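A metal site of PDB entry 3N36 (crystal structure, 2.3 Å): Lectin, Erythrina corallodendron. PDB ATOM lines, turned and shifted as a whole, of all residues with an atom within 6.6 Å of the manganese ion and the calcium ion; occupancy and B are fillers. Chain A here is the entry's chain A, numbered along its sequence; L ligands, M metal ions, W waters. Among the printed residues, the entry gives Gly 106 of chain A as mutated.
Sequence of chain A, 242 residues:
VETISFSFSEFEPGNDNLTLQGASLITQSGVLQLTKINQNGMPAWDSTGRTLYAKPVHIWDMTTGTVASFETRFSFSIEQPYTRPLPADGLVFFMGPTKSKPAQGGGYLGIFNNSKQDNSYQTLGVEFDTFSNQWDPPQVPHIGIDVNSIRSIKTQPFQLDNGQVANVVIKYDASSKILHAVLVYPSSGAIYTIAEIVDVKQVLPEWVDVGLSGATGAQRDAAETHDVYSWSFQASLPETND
O of Gly 144 is in hydrogen-bond range of N of Glu 127 (2.8 Å).
The calcium ion is bound by OD2 of Asp 136, O of Phe 131, water W3, OD1 of Asn 133, water W4, OD2 of Asp 129 and OD1 of Asp 129. The calcium ion has seven donor atoms within binding distance.
Water W2 lies within hydrogen-bond range of the backbone carbonyl oxygen of Ile 150 (2.6 Å), the side-chain carboxylate of Glu 127 (2.8 Å) and the indole nitrogen of Trp 135 (3.3 Å). Water W3 lies within hydrogen-bond range of O of Gly 107 and NE1 of Trp 135.
The manganese ion is bound by the side-chain carboxylate of Glu 127 (2.2 Å), the side-chain carboxylate of Asp 129 (2.3 Å), water W2 (2.4 Å), water W1 (2.4 Å), a ring nitrogen (NE2) of His 142 (2.4 Å) and the side-chain carboxylate of Asp 136 (2.4 Å). The manganese ion has six donor atoms within binding distance.
O4 of the ligand sits at hydrogen-bond distance from OD2 of Asp 89 (2.6 Å). An oxygen (O3) of the ligand lies within hydrogen-bond range of the backbone NH of Gly 107, 2.9 Å away. ND2 of Asn 133 is in hydrogen-bond range of O3 of the ligand (3.4 Å).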
ATOM      1  N   ASP A  89      15.329   1.587 -25.022  1.00  0.00           N
ATOM      2  CA  ASP A  89      14.251   0.692 -24.583  1.00  0.00           C
ATOM      3  C   ASP A  89      14.688  -0.097 -23.346  1.00  0.00           C
ATOM      4  O   ASP A  89      13.846  -0.591 -22.591  1.00  0.00           O
ATOM      5  CB  ASP A  89      13.904  -0.303 -25.686  1.00  0.00           C
ATOM      6  CG  ASP A  89      12.829   0.220 -26.615  1.00  0.00           C
ATOM      7  OD1 ASP A  89      11.675   0.338 -26.166  1.00  0.00           O
ATOM      8  OD2 ASP A  89      13.151   0.496 -27.789  1.00  0.00           O
ATOM      9  N   GLY A 106      14.246  -2.713 -30.398  1.00  0.00           N
ATOM     10  CA  GLY A 106      13.225  -1.906 -29.748  1.00  0.00           C
ATOM     11  C   GLY A 106      12.710  -2.519 -28.452  1.00  0.00           C
ATOM     12  O   GLY A 106      13.491  -3.026 -27.647  1.00  0.00           O
ATOM     13  N   GLY A 107      11.398  -2.462 -28.253  1.00  0.00           N
ATOM     14  CA  GLY A 107      10.807  -3.006 -27.043  1.00  0.00           C
ATOM     15  C   GLY A 107      11.008  -4.505 -26.815  1.00  0.00           C
ATOM     16  O   GLY A 107      10.681  -5.019 -25.753  1.00  0.00           O
ATOM     17  N   TYR A 108      11.533  -5.212 -27.812  1.00  0.00           N
ATOM     18  CA  TYR A 108      11.747  -6.658 -27.676  1.00  0.00           C
ATOM     19  C   TYR A 108      13.142  -6.947 -27.154  1.00  0.00           C
ATOM     20  O   TYR A 108      13.516  -8.103 -26.973  1.00  0.00           O
ATOM     21  CB  TYR A 108      11.498  -7.357 -29.011  1.00  0.00           C
ATOM     22  CG  TYR A 108      10.077  -7.206 -29.493  1.00  0.00           C
ATOM     23  CD1 TYR A 108       9.017  -7.684 -28.725  1.00  0.00           C
ATOM     24  CD2 TYR A 108       9.783  -6.523 -30.673  1.00  0.00           C
ATOM     25  CE1 TYR A 108       7.705  -7.503 -29.123  1.00  0.00           C
ATOM     26  CE2 TYR A 108       8.467  -6.337 -31.080  1.00  0.00           C
ATOM     27  CZ  TYR A 108       7.428  -6.821 -30.301  1.00  0.00           C
ATOM     28  OH  TYR A 108       6.129  -6.611 -30.691  1.00  0.00           O
ATOM     29  N   LEU A 109      13.892  -5.879 -26.914  1.00  0.00           N
ATOM     30  CA  LEU A 109      15.241  -5.944 -26.360  1.00  0.00           C
ATOM     31  C   LEU A 109      16.264  -6.866 -27.022  1.00  0.00           C
ATOM     32  O   LEU A 109      17.253  -7.258 -26.391  1.00  0.00           O
ATOM     33  CB  LEU A 109      15.152  -6.277 -24.864  1.00  0.00           C
ATOM     34  CG  LEU A 109      14.194  -5.359 -24.075  1.00  0.00           C
ATOM     35  CD1 LEU A 109      14.135  -5.813 -22.622  1.00  0.00           C
ATOM     36  CD2 LEU A 109      14.658  -3.909 -24.192  1.00  0.00           C
ATOM     37  N   GLU A 127      15.109  -8.183 -17.271  1.00  0.00           N
ATOM     38  CA  GLU A 127      15.194  -6.902 -17.955  1.00  0.00           C
ATOM     39  C   GLU A 127      15.238  -5.683 -17.058  1.00  0.00           C
ATOM     40  O   GLU A 127      14.884  -5.720 -15.864  1.00  0.00           O
ATOM     41  CB  GLU A 127      14.029  -6.751 -18.923  1.00  0.00           C
ATOM     42  CG  GLU A 127      12.697  -6.772 -18.166  1.00  0.00           C
ATOM     43  CD  GLU A 127      11.485  -6.410 -19.009  1.00  0.00           C
ATOM     44  OE1 GLU A 127      11.353  -6.881 -20.132  1.00  0.00           O
ATOM     45  OE2 GLU A 127      10.674  -5.607 -18.523  1.00  0.00           O
ATOM     46  N   ASP A 129      13.957  -2.352 -17.945  1.00  0.00           N
ATOM     47  CA  ASP A 129      13.104  -1.691 -18.930  1.00  0.00           C
ATOM     48  C   ASP A 129      12.862  -0.201 -18.726  1.00  0.00           C
ATOM     49  O   ASP A 129      12.251   0.192 -17.740  1.00  0.00           O
ATOM     50  CB  ASP A 129      11.746  -2.388 -18.937  1.00  0.00           C
ATOM     51  CG  ASP A 129      11.010  -2.229 -20.203  1.00  0.00           C
ATOM     52  OD1 ASP A 129      11.150  -1.176 -20.839  1.00  0.00           O
ATOM     53  OD2 ASP A 129      10.275  -3.183 -20.528  1.00  0.00           O
ATOM     54  N   THR A 130      13.224   0.549 -19.743  1.00  0.00           N
ATOM     55  CA  THR A 130      13.068   1.997 -19.645  1.00  0.00           C
ATOM     56  C   THR A 130      11.910   2.618 -20.439  1.00  0.00           C
ATOM     57  O   THR A 130      11.660   3.818 -20.312  1.00  0.00           O
ATOM     58  CB  THR A 130      14.366   2.692 -20.058  1.00  0.00           C
ATOM     59  OG1 THR A 130      14.694   2.310 -21.403  1.00  0.00           O
ATOM     60  CG2 THR A 130      15.505   2.297 -19.120  1.00  0.00           C
ATOM     61  N   PHE A 131      11.200   1.833 -21.250  1.00  0.00           N
ATOM     62  CA  PHE A 131      10.079   2.383 -22.015  1.00  0.00           C
ATOM     63  C   PHE A 131       8.830   1.582 -21.771  1.00  0.00           C
ATOM     64  O   PHE A 131       8.878   0.361 -21.790  1.00  0.00           O
ATOM     65  CB  PHE A 131      10.392   2.402 -23.511  1.00  0.00           C
ATOM     66  CG  PHE A 131       9.294   3.020 -24.351  1.00  0.00           C
ATOM     67  CD1 PHE A 131       9.230   4.405 -24.524  1.00  0.00           C
ATOM     68  CD2 PHE A 131       8.330   2.229 -24.956  1.00  0.00           C
ATOM     69  CE1 PHE A 131       8.198   4.987 -25.281  1.00  0.00           C
ATOM     70  CE2 PHE A 131       7.294   2.803 -25.727  1.00  0.00           C
ATOM     71  CZ  PHE A 131       7.241   4.191 -25.891  1.00  0.00           C
ATOM     72  N   SER A 132       7.701   2.247 -21.555  1.00  0.00           N
ATOM     73  CA  SER A 132       6.459   1.540 -21.291  1.00  0.00           C
ATOM     74  C   SER A 132       5.700   1.131 -22.575  1.00  0.00           C
ATOM     75  O   SER A 132       4.983   1.954 -23.143  1.00  0.00           O
ATOM     76  CB  SER A 132       5.548   2.399 -20.421  1.00  0.00           C
ATOM     77  OG  SER A 132       4.334   1.731 -20.138  1.00  0.00           O
ATOM     78  N   ASN A 133       5.873  -0.110 -23.009  1.00  0.00           N
ATOM     79  CA  ASN A 133       5.174  -0.628 -24.195  1.00  0.00           C
ATOM     80  C   ASN A 133       3.766  -1.055 -23.805  1.00  0.00           C
ATOM     81  O   ASN A 133       3.429  -1.065 -22.630  1.00  0.00           O
ATOM     82  CB  ASN A 133       5.896  -1.831 -24.799  1.00  0.00           C
ATOM     83  CG  ASN A 133       7.157  -1.433 -25.566  1.00  0.00           C
ATOM     84  OD1 ASN A 133       8.243  -1.467 -25.044  1.00  0.00           O
ATOM     85  ND2 ASN A 133       6.987  -1.056 -26.814  1.00  0.00           N
ATOM     86  N   TRP A 135       2.387  -3.922 -23.565  1.00  0.00           N
ATOM     87  CA  TRP A 135       2.334  -5.085 -22.697  1.00  0.00           C
ATOM     88  C   TRP A 135       2.976  -4.761 -21.347  1.00  0.00           C
ATOM     89  O   TRP A 135       3.020  -5.606 -20.459  1.00  0.00           O
ATOM     90  CB  TRP A 135       3.100  -6.242 -23.337  1.00  0.00           C
ATOM     91  CG  TRP A 135       4.520  -5.877 -23.717  1.00  0.00           C
ATOM     92  CD1 TRP A 135       5.618  -5.828 -22.907  1.00  0.00           C
ATOM     93  CD2 TRP A 135       4.990  -5.506 -25.032  1.00  0.00           C
ATOM     94  NE1 TRP A 135       6.732  -5.463 -23.613  1.00  0.00           N
ATOM     95  CE2 TRP A 135       6.371  -5.259 -24.929  1.00  0.00           C
ATOM     96  CE3 TRP A 135       4.367  -5.362 -26.278  1.00  0.00           C
ATOM     97  CZ2 TRP A 135       7.155  -4.869 -26.024  1.00  0.00           C
ATOM     98  CZ3 TRP A 135       5.138  -4.975 -27.368  1.00  0.00           C
ATOM     99  CH2 TRP A 135       6.515  -4.740 -27.244  1.00  0.00           C
ATOM    100  N   ASP A 136       3.476  -3.537 -21.203  1.00  0.00           N
ATOM    101  CA  ASP A 136       4.150  -3.132 -19.977  1.00  0.00           C
ATOM    102  C   ASP A 136       3.311  -2.444 -18.898  1.00  0.00           C
ATOM    103  O   ASP A 136       2.255  -1.880 -19.163  1.00  0.00           O
ATOM    104  CB  ASP A 136       5.305  -2.171 -20.296  1.00  0.00           C
ATOM    105  CG  ASP A 136       6.554  -2.872 -20.771  1.00  0.00           C
ATOM    106  OD1 ASP A 136       6.804  -4.033 -20.388  1.00  0.00           O
ATOM    107  OD2 ASP A 136       7.297  -2.237 -21.524  1.00  0.00           O
ATOM    108  N   PRO A 137       3.789  -2.528 -17.643  1.00  0.00           N
ATOM    109  CA  PRO A 137       3.060  -1.850 -16.566  1.00  0.00           C
ATOM    110  C   PRO A 137       3.386  -0.393 -16.895  1.00  0.00           C
ATOM    111  O   PRO A 137       4.378  -0.115 -17.571  1.00  0.00           O
ATOM    112  CB  PRO A 137       3.760  -2.338 -15.295  1.00  0.00           C
ATOM    113  CG  PRO A 137       5.144  -2.723 -15.772  1.00  0.00           C
ATOM    114  CD  PRO A 137       4.843  -3.394 -17.101  1.00  0.00           C
ATOM    115  N   VAL A 140       7.970   3.083 -15.409  1.00  0.00           N
ATOM    116  CA  VAL A 140       9.272   2.800 -15.987  1.00  0.00           C
ATOM    117  C   VAL A 140      10.253   3.762 -15.325  1.00  0.00           C
ATOM    118  O   VAL A 140       9.879   4.864 -14.960  1.00  0.00           O
ATOM    119  CB  VAL A 140       9.319   3.005 -17.518  1.00  0.00           C
ATOM    120  CG1 VAL A 140       8.629   1.859 -18.220  1.00  0.00           C
ATOM    121  CG2 VAL A 140       8.689   4.347 -17.891  1.00  0.00           C
ATOM    122  N   HIS A 142      11.558  -0.332 -14.912  1.00  0.00           N
ATOM    123  CA  HIS A 142      11.179  -1.420 -14.031  1.00  0.00           C
ATOM    124  C   HIS A 142      12.045  -2.622 -14.322  1.00  0.00           C
ATOM    125  O   HIS A 142      12.565  -2.777 -15.420  1.00  0.00           O
ATOM    126  CB  HIS A 142       9.692  -1.796 -14.172  1.00  0.00           C
ATOM    127  CG  HIS A 142       9.292  -2.204 -15.559  1.00  0.00           C
ATOM    128  ND1 HIS A 142       8.768  -1.324 -16.474  1.00  0.00           N
ATOM    129  CD2 HIS A 142       9.336  -3.411 -16.181  1.00  0.00           C
ATOM    130  CE1 HIS A 142       8.517  -1.955 -17.608  1.00  0.00           C
ATOM    131  NE2 HIS A 142       8.849  -3.229 -17.454  1.00  0.00           N
ATOM    132  N   ILE A 143      12.219  -3.446 -13.304  1.00  0.00           N
ATOM    133  CA  ILE A 143      12.987  -4.667 -13.440  1.00  0.00           C
ATOM    134  C   ILE A 143      11.918  -5.688 -13.787  1.00  0.00           C
ATOM    135  O   ILE A 143      10.771  -5.574 -13.344  1.00  0.00           O
ATOM    136  CB  ILE A 143      13.625  -5.090 -12.101  1.00  0.00           C
ATOM    137  CG1 ILE A 143      14.431  -3.930 -11.515  1.00  0.00           C
ATOM    138  CG2 ILE A 143      14.508  -6.325 -12.332  1.00  0.00           C
ATOM    139  CD1 ILE A 143      14.877  -4.187 -10.098  1.00  0.00           C
ATOM    140  N   GLY A 144      12.274  -6.684 -14.587  1.00  0.00           N
ATOM    141  CA  GLY A 144      11.300  -7.678 -14.932  1.00  0.00           C
ATOM    142  C   GLY A 144      11.891  -9.044 -15.140  1.00  0.00           C
ATOM    143  O   GLY A 144      13.027  -9.174 -15.599  1.00  0.00           O
ATOM    144  N   ASP A 146      11.435 -12.199 -17.261  1.00  0.00           N
ATOM    145  CA  ASP A 146      10.800 -12.646 -18.494  1.00  0.00           C
ATOM    146  C   ASP A 146      11.004 -14.130 -18.712  1.00  0.00           C
ATOM    147  O   ASP A 146      12.127 -14.626 -18.709  1.00  0.00           O
ATOM    148  CB  ASP A 146      11.359 -11.876 -19.691  1.00  0.00           C
ATOM    149  CG  ASP A 146      11.185 -10.365 -19.563  1.00  0.00           C
ATOM    150  OD1 ASP A 146      10.378  -9.941 -18.719  1.00  0.00           O
ATOM    151  OD2 ASP A 146      11.845  -9.615 -20.311  1.00  0.00           O
ATOM    152  N   ILE A 150       8.061 -11.285 -23.604  1.00  0.00           N
ATOM    153  CA  ILE A 150       8.525  -9.944 -23.253  1.00  0.00           C
ATOM    154  C   ILE A 150       7.596  -9.419 -22.152  1.00  0.00           C
ATOM    155  O   ILE A 150       7.945  -8.524 -21.392  1.00  0.00           O
ATOM    156  CB  ILE A 150       8.508  -9.011 -24.496  1.00  0.00           C
ATOM    157  CG1 ILE A 150       9.165  -7.669 -24.147  1.00  0.00           C
ATOM    158  CG2 ILE A 150       7.087  -8.808 -25.000  1.00  0.00           C
ATOM    159  CD1 ILE A 150      10.621  -7.772 -23.746  1.00  0.00           C
ATOM    160  N   ARG A 151       6.398  -9.998 -22.068  1.00  0.00           N
ATOM    161  CA  ARG A 151       5.436  -9.643 -21.029  1.00  0.00           C
ATOM    162  C   ARG A 151       5.881 -10.379 -19.756  1.00  0.00           C
ATOM    163  O   ARG A 151       5.730 -11.601 -19.645  1.00  0.00           O
ATOM    164  CB  ARG A 151       4.024 -10.094 -21.451  1.00  0.00           C
ATOM    165  CG  ARG A 151       2.938  -9.768 -20.426  1.00  0.00           C
ATOM    166  CD  ARG A 151       1.559 -10.245 -20.841  1.00  0.00           C
ATOM    167  NE  ARG A 151       0.813  -9.258 -21.632  1.00  0.00           N
ATOM    168  CZ  ARG A 151       0.896  -9.120 -22.955  1.00  0.00           C
ATOM    169  NH1 ARG A 151       1.690  -9.907 -23.673  1.00  0.00           N
ATOM    170  NH2 ARG A 151       0.175  -8.174 -23.568  1.00  0.00           N
ATOM    171  N   SER A 152       6.422  -9.633 -18.802  1.00  0.00           N
ATOM    172  CA  SER A 152       6.959 -10.194 -17.558  1.00  0.00           C
ATOM    173  C   SER A 152       5.965 -10.921 -16.647  1.00  0.00           C
ATOM    174  O   SER A 152       4.811 -10.529 -16.539  1.00  0.00           O
ATOM    175  CB  SER A 152       7.619  -9.079 -16.732  1.00  0.00           C
ATOM    176  OG  SER A 152       8.645  -8.426 -17.450  1.00  0.00           O
ATOM    177  N   THR A 155       7.210  -7.793 -12.189  1.00  0.00           N
ATOM    178  CA  THR A 155       7.985  -6.569 -12.342  1.00  0.00           C
ATOM    179  C   THR A 155       8.138  -5.792 -11.040  1.00  0.00           C
ATOM    180  O   THR A 155       7.313  -5.911 -10.128  1.00  0.00           O
ATOM    181  CB  THR A 155       7.344  -5.609 -13.365  1.00  0.00           C
ATOM    182  OG1 THR A 155       6.030  -5.261 -12.933  1.00  0.00           O
ATOM    183  CG2 THR A 155       7.288  -6.248 -14.745  1.00  0.00           C
HETATM  184  C1  LIG L   1       8.434   2.358 -30.755  1.00  0.00           C
HETATM  185  C2  LIG L   1       8.873   1.024 -30.165  1.00  0.00           C
HETATM  186  C3  LIG L   1       9.256   1.179 -28.692  1.00  0.00           C
HETATM  187  C4  LIG L   1      10.206   2.350 -28.490  1.00  0.00           C
HETATM  188  C5  LIG L   1       9.686   3.607 -29.180  1.00  0.00           C
HETATM  189  C6  LIG L   1      10.670   4.759 -29.043  1.00  0.00           C
HETATM  190  O1  LIG L   1       7.238   2.803 -30.095  1.00  0.00           O
HETATM  191  O2  LIG L   1       7.810   0.072 -30.289  1.00  0.00           O
HETATM  192  O3  LIG L   1       9.873  -0.023 -28.237  1.00  0.00           O
HETATM  193  O4  LIG L   1      11.492   2.011 -29.028  1.00  0.00           O
HETATM  194  O5  LIG L   1       9.464   3.328 -30.565  1.00  0.00           O
HETATM  195  O6  LIG L   1      10.016   5.988 -29.376  1.00  0.00           O
HETATM  196 MN    MN M   1       8.918  -4.662 -19.390  1.00  0.00          MN
HETATM  197 CA    CA M   2       9.321  -1.924 -22.716  1.00  0.00          CA
HETATM  198  O   HOH W   1       7.475  -6.037 -18.126  1.00  0.00           O
HETATM  199  O   HOH W   2       8.955  -6.089 -21.268  1.00  0.00           O
HETATM  200  O   HOH W   3       9.725  -4.430 -23.251  1.00  0.00           O
HETATM  201  O   HOH W   4      11.447  -0.974 -23.920  1.00  0.00           O
